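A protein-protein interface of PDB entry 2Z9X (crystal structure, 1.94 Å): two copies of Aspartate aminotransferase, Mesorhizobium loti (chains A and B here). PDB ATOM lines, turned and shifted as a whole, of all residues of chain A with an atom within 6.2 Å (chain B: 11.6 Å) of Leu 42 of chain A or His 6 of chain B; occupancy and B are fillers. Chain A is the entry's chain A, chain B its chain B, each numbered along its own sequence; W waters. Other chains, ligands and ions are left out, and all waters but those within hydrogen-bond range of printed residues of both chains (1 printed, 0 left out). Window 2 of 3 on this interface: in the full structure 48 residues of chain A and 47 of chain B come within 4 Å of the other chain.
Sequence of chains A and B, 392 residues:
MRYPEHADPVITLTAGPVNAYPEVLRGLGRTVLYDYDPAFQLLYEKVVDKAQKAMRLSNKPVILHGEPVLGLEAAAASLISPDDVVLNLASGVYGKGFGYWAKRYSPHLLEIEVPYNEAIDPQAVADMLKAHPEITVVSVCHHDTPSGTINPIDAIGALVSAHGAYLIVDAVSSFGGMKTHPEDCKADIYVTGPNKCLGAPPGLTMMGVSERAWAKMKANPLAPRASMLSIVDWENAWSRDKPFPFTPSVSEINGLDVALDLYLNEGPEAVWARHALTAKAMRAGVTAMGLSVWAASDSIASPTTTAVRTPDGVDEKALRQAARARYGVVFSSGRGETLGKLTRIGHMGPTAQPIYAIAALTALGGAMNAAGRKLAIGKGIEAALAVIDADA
The guanidinium group of Arg 324 of chain B lies within salt-bridge range of the side-chain carboxylate of Asp 37 of chain A (2.8 Å). The backbone carbonyl oxygen of Glu 5 of chain B is in hydrogen-bond range of the backbone NH of Ala 39 of chain A.
N of Ala 39 of chain A lies within hydrogen-bond range of OD1 of Asp 37 of chain A, 2.8 Å away. O of Pro 4 of chain B is in hydrogen-bond range of NH1 of Arg 324 of chain B. O of Ala 7 of chain B lies within hydrogen-bond range of NH2 of Arg 324 of chain B, 2.8 Å away.
Among the printed residues, pairs that only touch across the chains: Asp 37 of chain A with Pro 9 of chain B (3.6 Å), Asp 37 of chain A with Val 330 of chain B (3.3 Å), Pro 38 of chain A with Glu 5 of chain B (3.5 Å), Pro 38 of chain A with Arg 324 of chain B (3.7 Å), Ala 39 of chain A with His 6 of chain B (3.6 Å), Ala 39 of chain A with Ala 7 of chain B (3.7 Å), Ala 39 of chain A with Arg 324 of chain B (3.7 Å) and Leu 42 of chain A with His 6 of chain B (3.8 Å).
Leu 42 of chain A touches just one residue of chain B: His 6. His 6 of chain B touches two residues of chain A. No residue of chain B comes within 4 Å of Gln 41 of chain A. No residue of chain B comes within 4 Å of Glu 45 of chain A. No residue of chain B comes within 4 Å of Arg 240 of chain A. Of the printed residues of chain A, Val 330 of chain B touches Asp 37 (3.3 Å). Of the printed residues of chain A, Pro 9 of chain B touches Asp 37 (3.6 Å). Of the printed residues of chain A, Ala 7 of chain B touches Ala 39. Val 10 of chain B touches none of the printed residues of chain A. Lys 46 of chain A touches none of the printed residues of chain B. The nearest residue of chain A that does not touch His 6 of chain B is Pro 38 of chain A (5.3 Å).
Of the 14 printed residues of chain B, 6 touch a printed residue of chain A. Printed residues of chain B that touch a printed residue of chain A: Glu 5, His 6, Ala 7, Pro 9, Arg 324 and Val 330. Hydrophobic or aromatic side chains of chain B that line the printed part of chain A: His 6, Pro 9 and Val 330. Hydrophobic or aromatic side chains of chain A that line the printed part of chain B: Pro 38, Ala 39 and Leu 42. Among the printed residues, 10 pairs touch across the chains. Among the printed residues, Asp or Glu carboxylates within 4 Å of a Lys or Arg side-chain nitrogen of the other chain: Asp 37 of chain A with Arg 324 of chain B.
No position is printed for both chains.
Water W1 lies within hydrogen-bond range of O of Ala 39 of chain A (2.8 Å) and O of His 6 of chain B (3.3 Å).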
ATOM      1  N   ASP A  37       0.250  -6.718 -17.872  1.00  0.00           N
ATOM      2  CA  ASP A  37       0.824  -7.907 -18.499  1.00  0.00           C
ATOM      3  C   ASP A  37       0.692  -7.718 -20.017  1.00  0.00           C
ATOM      4  O   ASP A  37      -0.382  -7.341 -20.497  1.00  0.00           O
ATOM      5  CB  ASP A  37       0.077  -9.155 -18.048  1.00  0.00           C
ATOM      6  CG  ASP A  37       0.757 -10.424 -18.488  1.00  0.00           C
ATOM      7  OD1 ASP A  37       0.685 -10.762 -19.693  1.00  0.00           O
ATOM      8  OD2 ASP A  37       1.381 -11.087 -17.636  1.00  0.00           O
ATOM      9  N   PRO A  38       1.778  -7.946 -20.778  1.00  0.00           N
ATOM     10  CA  PRO A  38       1.693  -7.739 -22.224  1.00  0.00           C
ATOM     11  C   PRO A  38       0.613  -8.605 -22.894  1.00  0.00           C
ATOM     12  O   PRO A  38       0.076  -8.201 -23.933  1.00  0.00           O
ATOM     13  CB  PRO A  38       3.090  -8.125 -22.722  1.00  0.00           C
ATOM     14  CG  PRO A  38       3.637  -9.031 -21.657  1.00  0.00           C
ATOM     15  CD  PRO A  38       3.116  -8.421 -20.382  1.00  0.00           C
ATOM     16  N   ALA A  39       0.297  -9.761 -22.312  1.00  0.00           N
ATOM     17  CA  ALA A  39      -0.760 -10.621 -22.855  1.00  0.00           C
ATOM     18  C   ALA A  39      -2.137  -9.984 -22.687  1.00  0.00           C
ATOM     19  O   ALA A  39      -3.004 -10.136 -23.545  1.00  0.00           O
ATOM     20  CB  ALA A  39      -0.724 -12.030 -22.212  1.00  0.00           C
ATOM     21  N   PHE A  40      -2.341  -9.277 -21.576  1.00  0.00           N
ATOM     22  CA  PHE A  40      -3.606  -8.572 -21.395  1.00  0.00           C
ATOM     23  C   PHE A  40      -3.671  -7.321 -22.240  1.00  0.00           C
ATOM     24  O   PHE A  40      -4.713  -7.014 -22.797  1.00  0.00           O
ATOM     25  CB  PHE A  40      -3.911  -8.201 -19.945  1.00  0.00           C
ATOM     26  CG  PHE A  40      -5.284  -7.603 -19.787  1.00  0.00           C
ATOM     27  CD1 PHE A  40      -5.452  -6.227 -19.762  1.00  0.00           C
ATOM     28  CD2 PHE A  40      -6.421  -8.428 -19.746  1.00  0.00           C
ATOM     29  CE1 PHE A  40      -6.713  -5.654 -19.646  1.00  0.00           C
ATOM     30  CE2 PHE A  40      -7.708  -7.860 -19.635  1.00  0.00           C
ATOM     31  CZ  PHE A  40      -7.851  -6.487 -19.596  1.00  0.00           C
ATOM     32  N   GLN A  41      -2.551  -6.597 -22.335  1.00  0.00           N
ATOM     33  CA  GLN A  41      -2.483  -5.406 -23.179  1.00  0.00           C
ATOM     34  C   GLN A  41      -2.867  -5.767 -24.612  1.00  0.00           C
ATOM     35  O   GLN A  41      -3.620  -5.042 -25.272  1.00  0.00           O
ATOM     36  CB  GLN A  41      -1.068  -4.837 -23.139  1.00  0.00           C
ATOM     37  CG  GLN A  41      -0.736  -4.171 -21.788  1.00  0.00           C
ATOM     38  CD  GLN A  41      -1.324  -2.768 -21.680  1.00  0.00           C
ATOM     39  OE1 GLN A  41      -2.416  -2.488 -22.198  1.00  0.00           O
ATOM     40  NE2 GLN A  41      -0.598  -1.873 -21.016  1.00  0.00           N
ATOM     41  N   LEU A  42      -2.341  -6.900 -25.076  1.00  0.00           N
ATOM     42  CA  LEU A  42      -2.660  -7.366 -26.434  1.00  0.00           C
ATOM     43  C   LEU A  42      -4.148  -7.727 -26.558  1.00  0.00           C
ATOM     44  O   LEU A  42      -4.840  -7.322 -27.516  1.00  0.00           O
ATOM     45  CB  LEU A  42      -1.776  -8.555 -26.801  1.00  0.00           C
ATOM     46  CG  LEU A  42      -2.007  -9.087 -28.217  1.00  0.00           C
ATOM     47  CD1 LEU A  42      -1.820  -7.959 -29.251  1.00  0.00           C
ATOM     48  CD2 LEU A  42      -1.071 -10.266 -28.480  1.00  0.00           C
ATOM     49  N   LEU A  43      -4.633  -8.504 -25.587  1.00  0.00           N
ATOM     50  CA  LEU A  43      -6.032  -8.923 -25.566  1.00  0.00           C
ATOM     51  C   LEU A  43      -6.958  -7.719 -25.605  1.00  0.00           C
ATOM     52  O   LEU A  43      -7.919  -7.695 -26.394  1.00  0.00           O
ATOM     53  CB  LEU A  43      -6.361  -9.782 -24.335  1.00  0.00           C
ATOM     54  CG  LEU A  43      -7.865 -10.031 -24.121  1.00  0.00           C
ATOM     55  CD1 LEU A  43      -8.357 -11.108 -25.110  1.00  0.00           C
ATOM     56  CD2 LEU A  43      -8.196 -10.414 -22.671  1.00  0.00           C
ATOM     57  N   TYR A  44      -6.688  -6.722 -24.743  1.00  0.00           N
ATOM     58  CA  TYR A  44      -7.546  -5.530 -24.680  1.00  0.00           C
ATOM     59  C   TYR A  44      -7.596  -4.829 -26.042  1.00  0.00           C
ATOM     60  O   TYR A  44      -8.658  -4.418 -26.508  1.00  0.00           O
ATOM     61  CB  TYR A  44      -7.062  -4.538 -23.610  1.00  0.00           C
ATOM     62  CG  TYR A  44      -8.071  -3.482 -23.242  1.00  0.00           C
ATOM     63  CD1 TYR A  44      -8.150  -2.273 -23.956  1.00  0.00           C
ATOM     64  CD2 TYR A  44      -8.956  -3.680 -22.167  1.00  0.00           C
ATOM     65  CE1 TYR A  44      -9.082  -1.312 -23.627  1.00  0.00           C
ATOM     66  CE2 TYR A  44      -9.874  -2.705 -21.816  1.00  0.00           C
ATOM     67  CZ  TYR A  44      -9.937  -1.519 -22.550  1.00  0.00           C
ATOM     68  OH  TYR A  44     -10.866  -0.544 -22.215  1.00  0.00           O
ATOM     69  N   GLU A  45      -6.426  -4.666 -26.658  1.00  0.00           N
ATOM     70  CA  GLU A  45      -6.366  -4.081 -27.989  1.00  0.00           C
ATOM     71  C   GLU A  45      -7.209  -4.869 -28.997  1.00  0.00           C
ATOM     72  O   GLU A  45      -7.961  -4.270 -29.786  1.00  0.00           O
ATOM     73  CB  GLU A  45      -4.923  -4.003 -28.481  1.00  0.00           C
ATOM     74  CG  GLU A  45      -4.829  -3.209 -29.795  1.00  0.00           C
ATOM     75  CD  GLU A  45      -3.419  -2.991 -30.265  1.00  0.00           C
ATOM     76  OE1 GLU A  45      -2.547  -2.580 -29.469  1.00  0.00           O
ATOM     77  OE2 GLU A  45      -3.179  -3.216 -31.462  1.00  0.00           O
ATOM     78  N   LYS A  46      -7.083  -6.202 -28.956  1.00  0.00           N
ATOM     79  CA  LYS A  46      -7.821  -7.043 -29.890  1.00  0.00           C
ATOM     80  C   LYS A  46      -9.328  -7.022 -29.630  1.00  0.00           C
ATOM     81  O   LYS A  46     -10.117  -7.103 -30.579  1.00  0.00           O
ATOM     82  CB  LYS A  46      -7.259  -8.470 -29.917  1.00  0.00           C
ATOM     83  CG  LYS A  46      -5.785  -8.545 -30.386  1.00  0.00           C
ATOM     84  CD  LYS A  46      -5.592  -8.122 -31.851  1.00  0.00           C
ATOM     85  CE  LYS A  46      -4.136  -8.300 -32.288  1.00  0.00           C
ATOM     86  NZ  LYS A  46      -3.825  -7.647 -33.595  1.00  0.00           N
ATOM     87  N   VAL A  47      -9.733  -6.873 -28.369  1.00  0.00           N
ATOM     88  CA  VAL A  47     -11.165  -6.738 -28.056  1.00  0.00           C
ATOM     89  C   VAL A  47     -11.740  -5.457 -28.652  1.00  0.00           C
ATOM     90  O   VAL A  47     -12.868  -5.454 -29.190  1.00  0.00           O
ATOM     91  CB  VAL A  47     -11.454  -6.793 -26.513  1.00  0.00           C
ATOM     92  CG1 VAL A  47     -12.882  -6.372 -26.210  1.00  0.00           C
ATOM     93  CG2 VAL A  47     -11.245  -8.217 -25.987  1.00  0.00           C
ATOM     94  N   ARG A 240      -2.040  -1.371 -26.925  1.00  0.00           N
ATOM     95  CA  ARG A 240      -1.187  -2.220 -26.082  1.00  0.00           C
ATOM     96  C   ARG A 240       0.024  -1.463 -25.496  1.00  0.00           C
ATOM     97  O   ARG A 240       0.632  -1.927 -24.514  1.00  0.00           O
ATOM     98  CB  ARG A 240      -0.691  -3.445 -26.882  1.00  0.00           C
ATOM     99  CG  ARG A 240       0.460  -3.093 -27.872  1.00  0.00           C
ATOM    100  CD  ARG A 240       0.821  -4.228 -28.820  1.00  0.00           C
ATOM    101  NE  ARG A 240      -0.155  -4.343 -29.896  1.00  0.00           N
ATOM    102  CZ  ARG A 240      -0.066  -5.199 -30.910  1.00  0.00           C
ATOM    103  NH1 ARG A 240       0.971  -6.017 -31.007  1.00  0.00           N
ATOM    104  NH2 ARG A 240      -1.022  -5.241 -31.831  1.00  0.00           N
ATOM    105  N   ARG B   2      12.237 -19.091 -23.375  1.00  0.00           N
ATOM    106  CA  ARG B   2      11.735 -17.739 -23.164  1.00  0.00           C
ATOM    107  C   ARG B   2      10.219 -17.710 -23.338  1.00  0.00           C
ATOM    108  O   ARG B   2       9.665 -18.302 -24.270  1.00  0.00           O
ATOM    109  CB  ARG B   2      12.409 -16.730 -24.110  1.00  0.00           C
ATOM    110  CG  ARG B   2      13.929 -16.494 -23.884  1.00  0.00           C
ATOM    111  CD  ARG B   2      14.260 -15.902 -22.500  1.00  0.00           C
ATOM    112  NE  ARG B   2      15.686 -15.607 -22.365  1.00  0.00           N
ATOM    113  CZ  ARG B   2      16.223 -14.401 -22.505  1.00  0.00           C
ATOM    114  NH1 ARG B   2      17.536 -14.242 -22.369  1.00  0.00           N
ATOM    115  NH2 ARG B   2      15.457 -13.350 -22.787  1.00  0.00           N
ATOM    116  N   TYR B   3       9.550 -17.018 -22.413  1.00  0.00           N
ATOM    117  CA  TYR B   3       8.109 -16.888 -22.442  1.00  0.00           C
ATOM    118  C   TYR B   3       7.705 -15.749 -23.379  1.00  0.00           C
ATOM    119  O   TYR B   3       8.058 -14.592 -23.137  1.00  0.00           O
ATOM    120  CB  TYR B   3       7.565 -16.659 -21.019  1.00  0.00           C
ATOM    121  CG  TYR B   3       7.730 -17.884 -20.139  1.00  0.00           C
ATOM    122  CD1 TYR B   3       8.871 -18.060 -19.348  1.00  0.00           C
ATOM    123  CD2 TYR B   3       6.762 -18.893 -20.140  1.00  0.00           C
ATOM    124  CE1 TYR B   3       9.031 -19.209 -18.551  1.00  0.00           C
ATOM    125  CE2 TYR B   3       6.911 -20.034 -19.367  1.00  0.00           C
ATOM    126  CZ  TYR B   3       8.034 -20.184 -18.561  1.00  0.00           C
ATOM    127  OH  TYR B   3       8.155 -21.333 -17.818  1.00  0.00           O
ATOM    128  N   PRO B   4       6.950 -16.069 -24.450  1.00  0.00           N
ATOM    129  CA  PRO B   4       6.512 -14.982 -25.330  1.00  0.00           C
ATOM    130  C   PRO B   4       5.602 -13.976 -24.620  1.00  0.00           C
ATOM    131  O   PRO B   4       4.793 -14.352 -23.781  1.00  0.00           O
ATOM    132  CB  PRO B   4       5.735 -15.698 -26.437  1.00  0.00           C
ATOM    133  CG  PRO B   4       6.135 -17.154 -26.348  1.00  0.00           C
ATOM    134  CD  PRO B   4       6.469 -17.389 -24.901  1.00  0.00           C
ATOM    135  N   GLU B   5       5.716 -12.710 -24.995  1.00  0.00           N
ATOM    136  CA  GLU B   5       4.860 -11.654 -24.436  1.00  0.00           C
ATOM    137  C   GLU B   5       3.367 -11.876 -24.688  1.00  0.00           C
ATOM    138  O   GLU B   5       2.532 -11.487 -23.862  1.00  0.00           O
ATOM    139  CB  GLU B   5       5.286 -10.278 -24.963  1.00  0.00           C
ATOM    140  CG  GLU B   5       6.618  -9.835 -24.389  1.00  0.00           C
ATOM    141  CD  GLU B   5       6.994  -8.429 -24.793  1.00  0.00           C
ATOM    142  OE1 GLU B   5       6.198  -7.766 -25.489  1.00  0.00           O
ATOM    143  OE2 GLU B   5       8.097  -7.985 -24.405  1.00  0.00           O
ATOM    144  N   HIS B   6       3.039 -12.516 -25.810  1.00  0.00           N
ATOM    145  CA  HIS B   6       1.633 -12.736 -26.199  1.00  0.00           C
ATOM    146  C   HIS B   6       1.000 -13.911 -25.447  1.00  0.00           C
ATOM    147  O   HIS B   6      -0.209 -13.950 -25.267  1.00  0.00           O
ATOM    148  CB  HIS B   6       1.508 -12.956 -27.718  1.00  0.00           C
ATOM    149  CG  HIS B   6       1.872 -14.351 -28.164  1.00  0.00           C
ATOM    150  ND1 HIS B   6       3.117 -14.674 -28.669  1.00  0.00           N
ATOM    151  CD2 HIS B   6       1.156 -15.504 -28.165  1.00  0.00           C
ATOM    152  CE1 HIS B   6       3.150 -15.963 -28.964  1.00  0.00           C
ATOM    153  NE2 HIS B   6       1.974 -16.490 -28.660  1.00  0.00           N
ATOM    154  N   ALA B   7       1.821 -14.861 -25.012  1.00  0.00           N
ATOM    155  CA  ALA B   7       1.340 -16.057 -24.324  1.00  0.00           C
ATOM    156  C   ALA B   7       1.121 -15.742 -22.837  1.00  0.00           C
ATOM    157  O   ALA B   7       1.738 -14.830 -22.298  1.00  0.00           O
ATOM    158  CB  ALA B   7       2.338 -17.191 -24.491  1.00  0.00           C
ATOM    159  N   ASP B   8       0.238 -16.489 -22.186  1.00  0.00           N
ATOM    160  CA  ASP B   8      -0.048 -16.273 -20.761  1.00  0.00           C
ATOM    161  C   ASP B   8       1.192 -16.571 -19.913  1.00  0.00           C
ATOM    162  O   ASP B   8       2.035 -17.365 -20.316  1.00  0.00           O
ATOM    163  CB  ASP B   8      -1.263 -17.115 -20.310  1.00  0.00           C
ATOM    164  CG  ASP B   8      -2.596 -16.363 -20.476  1.00  0.00           C
ATOM    165  OD1 ASP B   8      -2.693 -15.488 -21.363  1.00  0.00           O
ATOM    166  OD2 ASP B   8      -3.557 -16.641 -19.706  1.00  0.00           O
ATOM    167  N   PRO B   9       1.336 -15.898 -18.743  1.00  0.00           N
ATOM    168  CA  PRO B   9       2.503 -16.183 -17.903  1.00  0.00           C
ATOM    169  C   PRO B   9       2.258 -17.420 -17.043  1.00  0.00           C
ATOM    170  O   PRO B   9       1.181 -18.033 -17.136  1.00  0.00           O
ATOM    171  CB  PRO B   9       2.570 -14.960 -17.008  1.00  0.00           C
ATOM    172  CG  PRO B   9       1.077 -14.593 -16.821  1.00  0.00           C
ATOM    173  CD  PRO B   9       0.468 -14.851 -18.161  1.00  0.00           C
ATOM    174  N   VAL B  10       3.226 -17.761 -16.184  1.00  0.00           N
ATOM    175  CA  VAL B  10       3.106 -18.935 -15.316  1.00  0.00           C
ATOM    176  C   VAL B  10       2.528 -18.581 -13.960  1.00  0.00           C
ATOM    177  O   VAL B  10       1.603 -19.244 -13.488  1.00  0.00           O
ATOM    178  CB  VAL B  10       4.430 -19.692 -15.181  1.00  0.00           C
ATOM    179  CG1 VAL B  10       4.241 -20.929 -14.274  1.00  0.00           C
ATOM    180  CG2 VAL B  10       4.896 -20.133 -16.580  1.00  0.00           C
ATOM    181  N   GLN B 321      10.466  -7.199 -17.223  1.00  0.00           N
ATOM    182  CA  GLN B 321      10.388  -7.898 -18.515  1.00  0.00           C
ATOM    183  C   GLN B 321      11.207  -9.186 -18.526  1.00  0.00           C
ATOM    184  O   GLN B 321      10.776 -10.210 -19.073  1.00  0.00           O
ATOM    185  CB  GLN B 321      10.868  -6.961 -19.613  1.00  0.00           C
ATOM    186  CG  GLN B 321       9.854  -5.866 -19.947  1.00  0.00           C
ATOM    187  CD  GLN B 321      10.375  -4.893 -20.993  1.00  0.00           C
ATOM    188  OE1 GLN B 321       9.588  -4.239 -21.687  1.00  0.00           O
ATOM    189  NE2 GLN B 321      11.700  -4.773 -21.094  1.00  0.00           N
ATOM    190  N   ARG B 324       9.533 -12.025 -16.336  1.00  0.00           N
ATOM    191  CA  ARG B 324       8.473 -12.701 -17.104  1.00  0.00           C
ATOM    192  C   ARG B 324       9.028 -13.566 -18.245  1.00  0.00           C
ATOM    193  O   ARG B 324       8.634 -14.716 -18.384  1.00  0.00           O
ATOM    194  CB  ARG B 324       7.461 -11.691 -17.669  1.00  0.00           C
ATOM    195  CG  ARG B 324       6.194 -12.373 -18.186  1.00  0.00           C
ATOM    196  CD  ARG B 324       5.271 -11.320 -18.795  1.00  0.00           C
ATOM    197  NE  ARG B 324       3.927 -11.803 -19.106  1.00  0.00           N
ATOM    198  CZ  ARG B 324       3.611 -12.584 -20.144  1.00  0.00           C
ATOM    199  NH1 ARG B 324       4.546 -13.059 -20.957  1.00  0.00           N
ATOM    200  NH2 ARG B 324       2.344 -12.904 -20.361  1.00  0.00           N
ATOM    201  N   ALA B 325       9.942 -13.008 -19.050  1.00  0.00           N
ATOM    202  CA  ALA B 325      10.497 -13.720 -20.202  1.00  0.00           C
ATOM    203  C   ALA B 325      11.282 -14.947 -19.790  1.00  0.00           C
ATOM    204  O   ALA B 325      11.221 -15.962 -20.465  1.00  0.00           O
ATOM    205  CB  ALA B 325      11.393 -12.800 -21.062  1.00  0.00           C
ATOM    206  N   GLY B 328       8.580 -16.680 -16.297  1.00  0.00           N
ATOM    207  CA  GLY B 328       7.129 -16.732 -16.404  1.00  0.00           C
ATOM    208  C   GLY B 328       6.428 -16.102 -15.223  1.00  0.00           C
ATOM    209  O   GLY B 328       5.230 -16.319 -15.024  1.00  0.00           O
ATOM    210  N   VAL B 330       5.248 -12.701 -13.071  1.00  0.00           N
ATOM    211  CA  VAL B 330       4.897 -11.302 -13.351  1.00  0.00           C
ATOM    212  C   VAL B 330       4.846 -10.503 -12.075  1.00  0.00           C
ATOM    213  O   VAL B 330       4.145 -10.881 -11.126  1.00  0.00           O
ATOM    214  CB  VAL B 330       3.533 -11.170 -14.078  1.00  0.00           C
ATOM    215  CG1 VAL B 330       3.253  -9.689 -14.481  1.00  0.00           C
ATOM    216  CG2 VAL B 330       3.490 -12.094 -15.286  1.00  0.00           C
HETATM  217  O   HOH W   1      -3.081 -12.289 -25.279  1.00  0.00           O
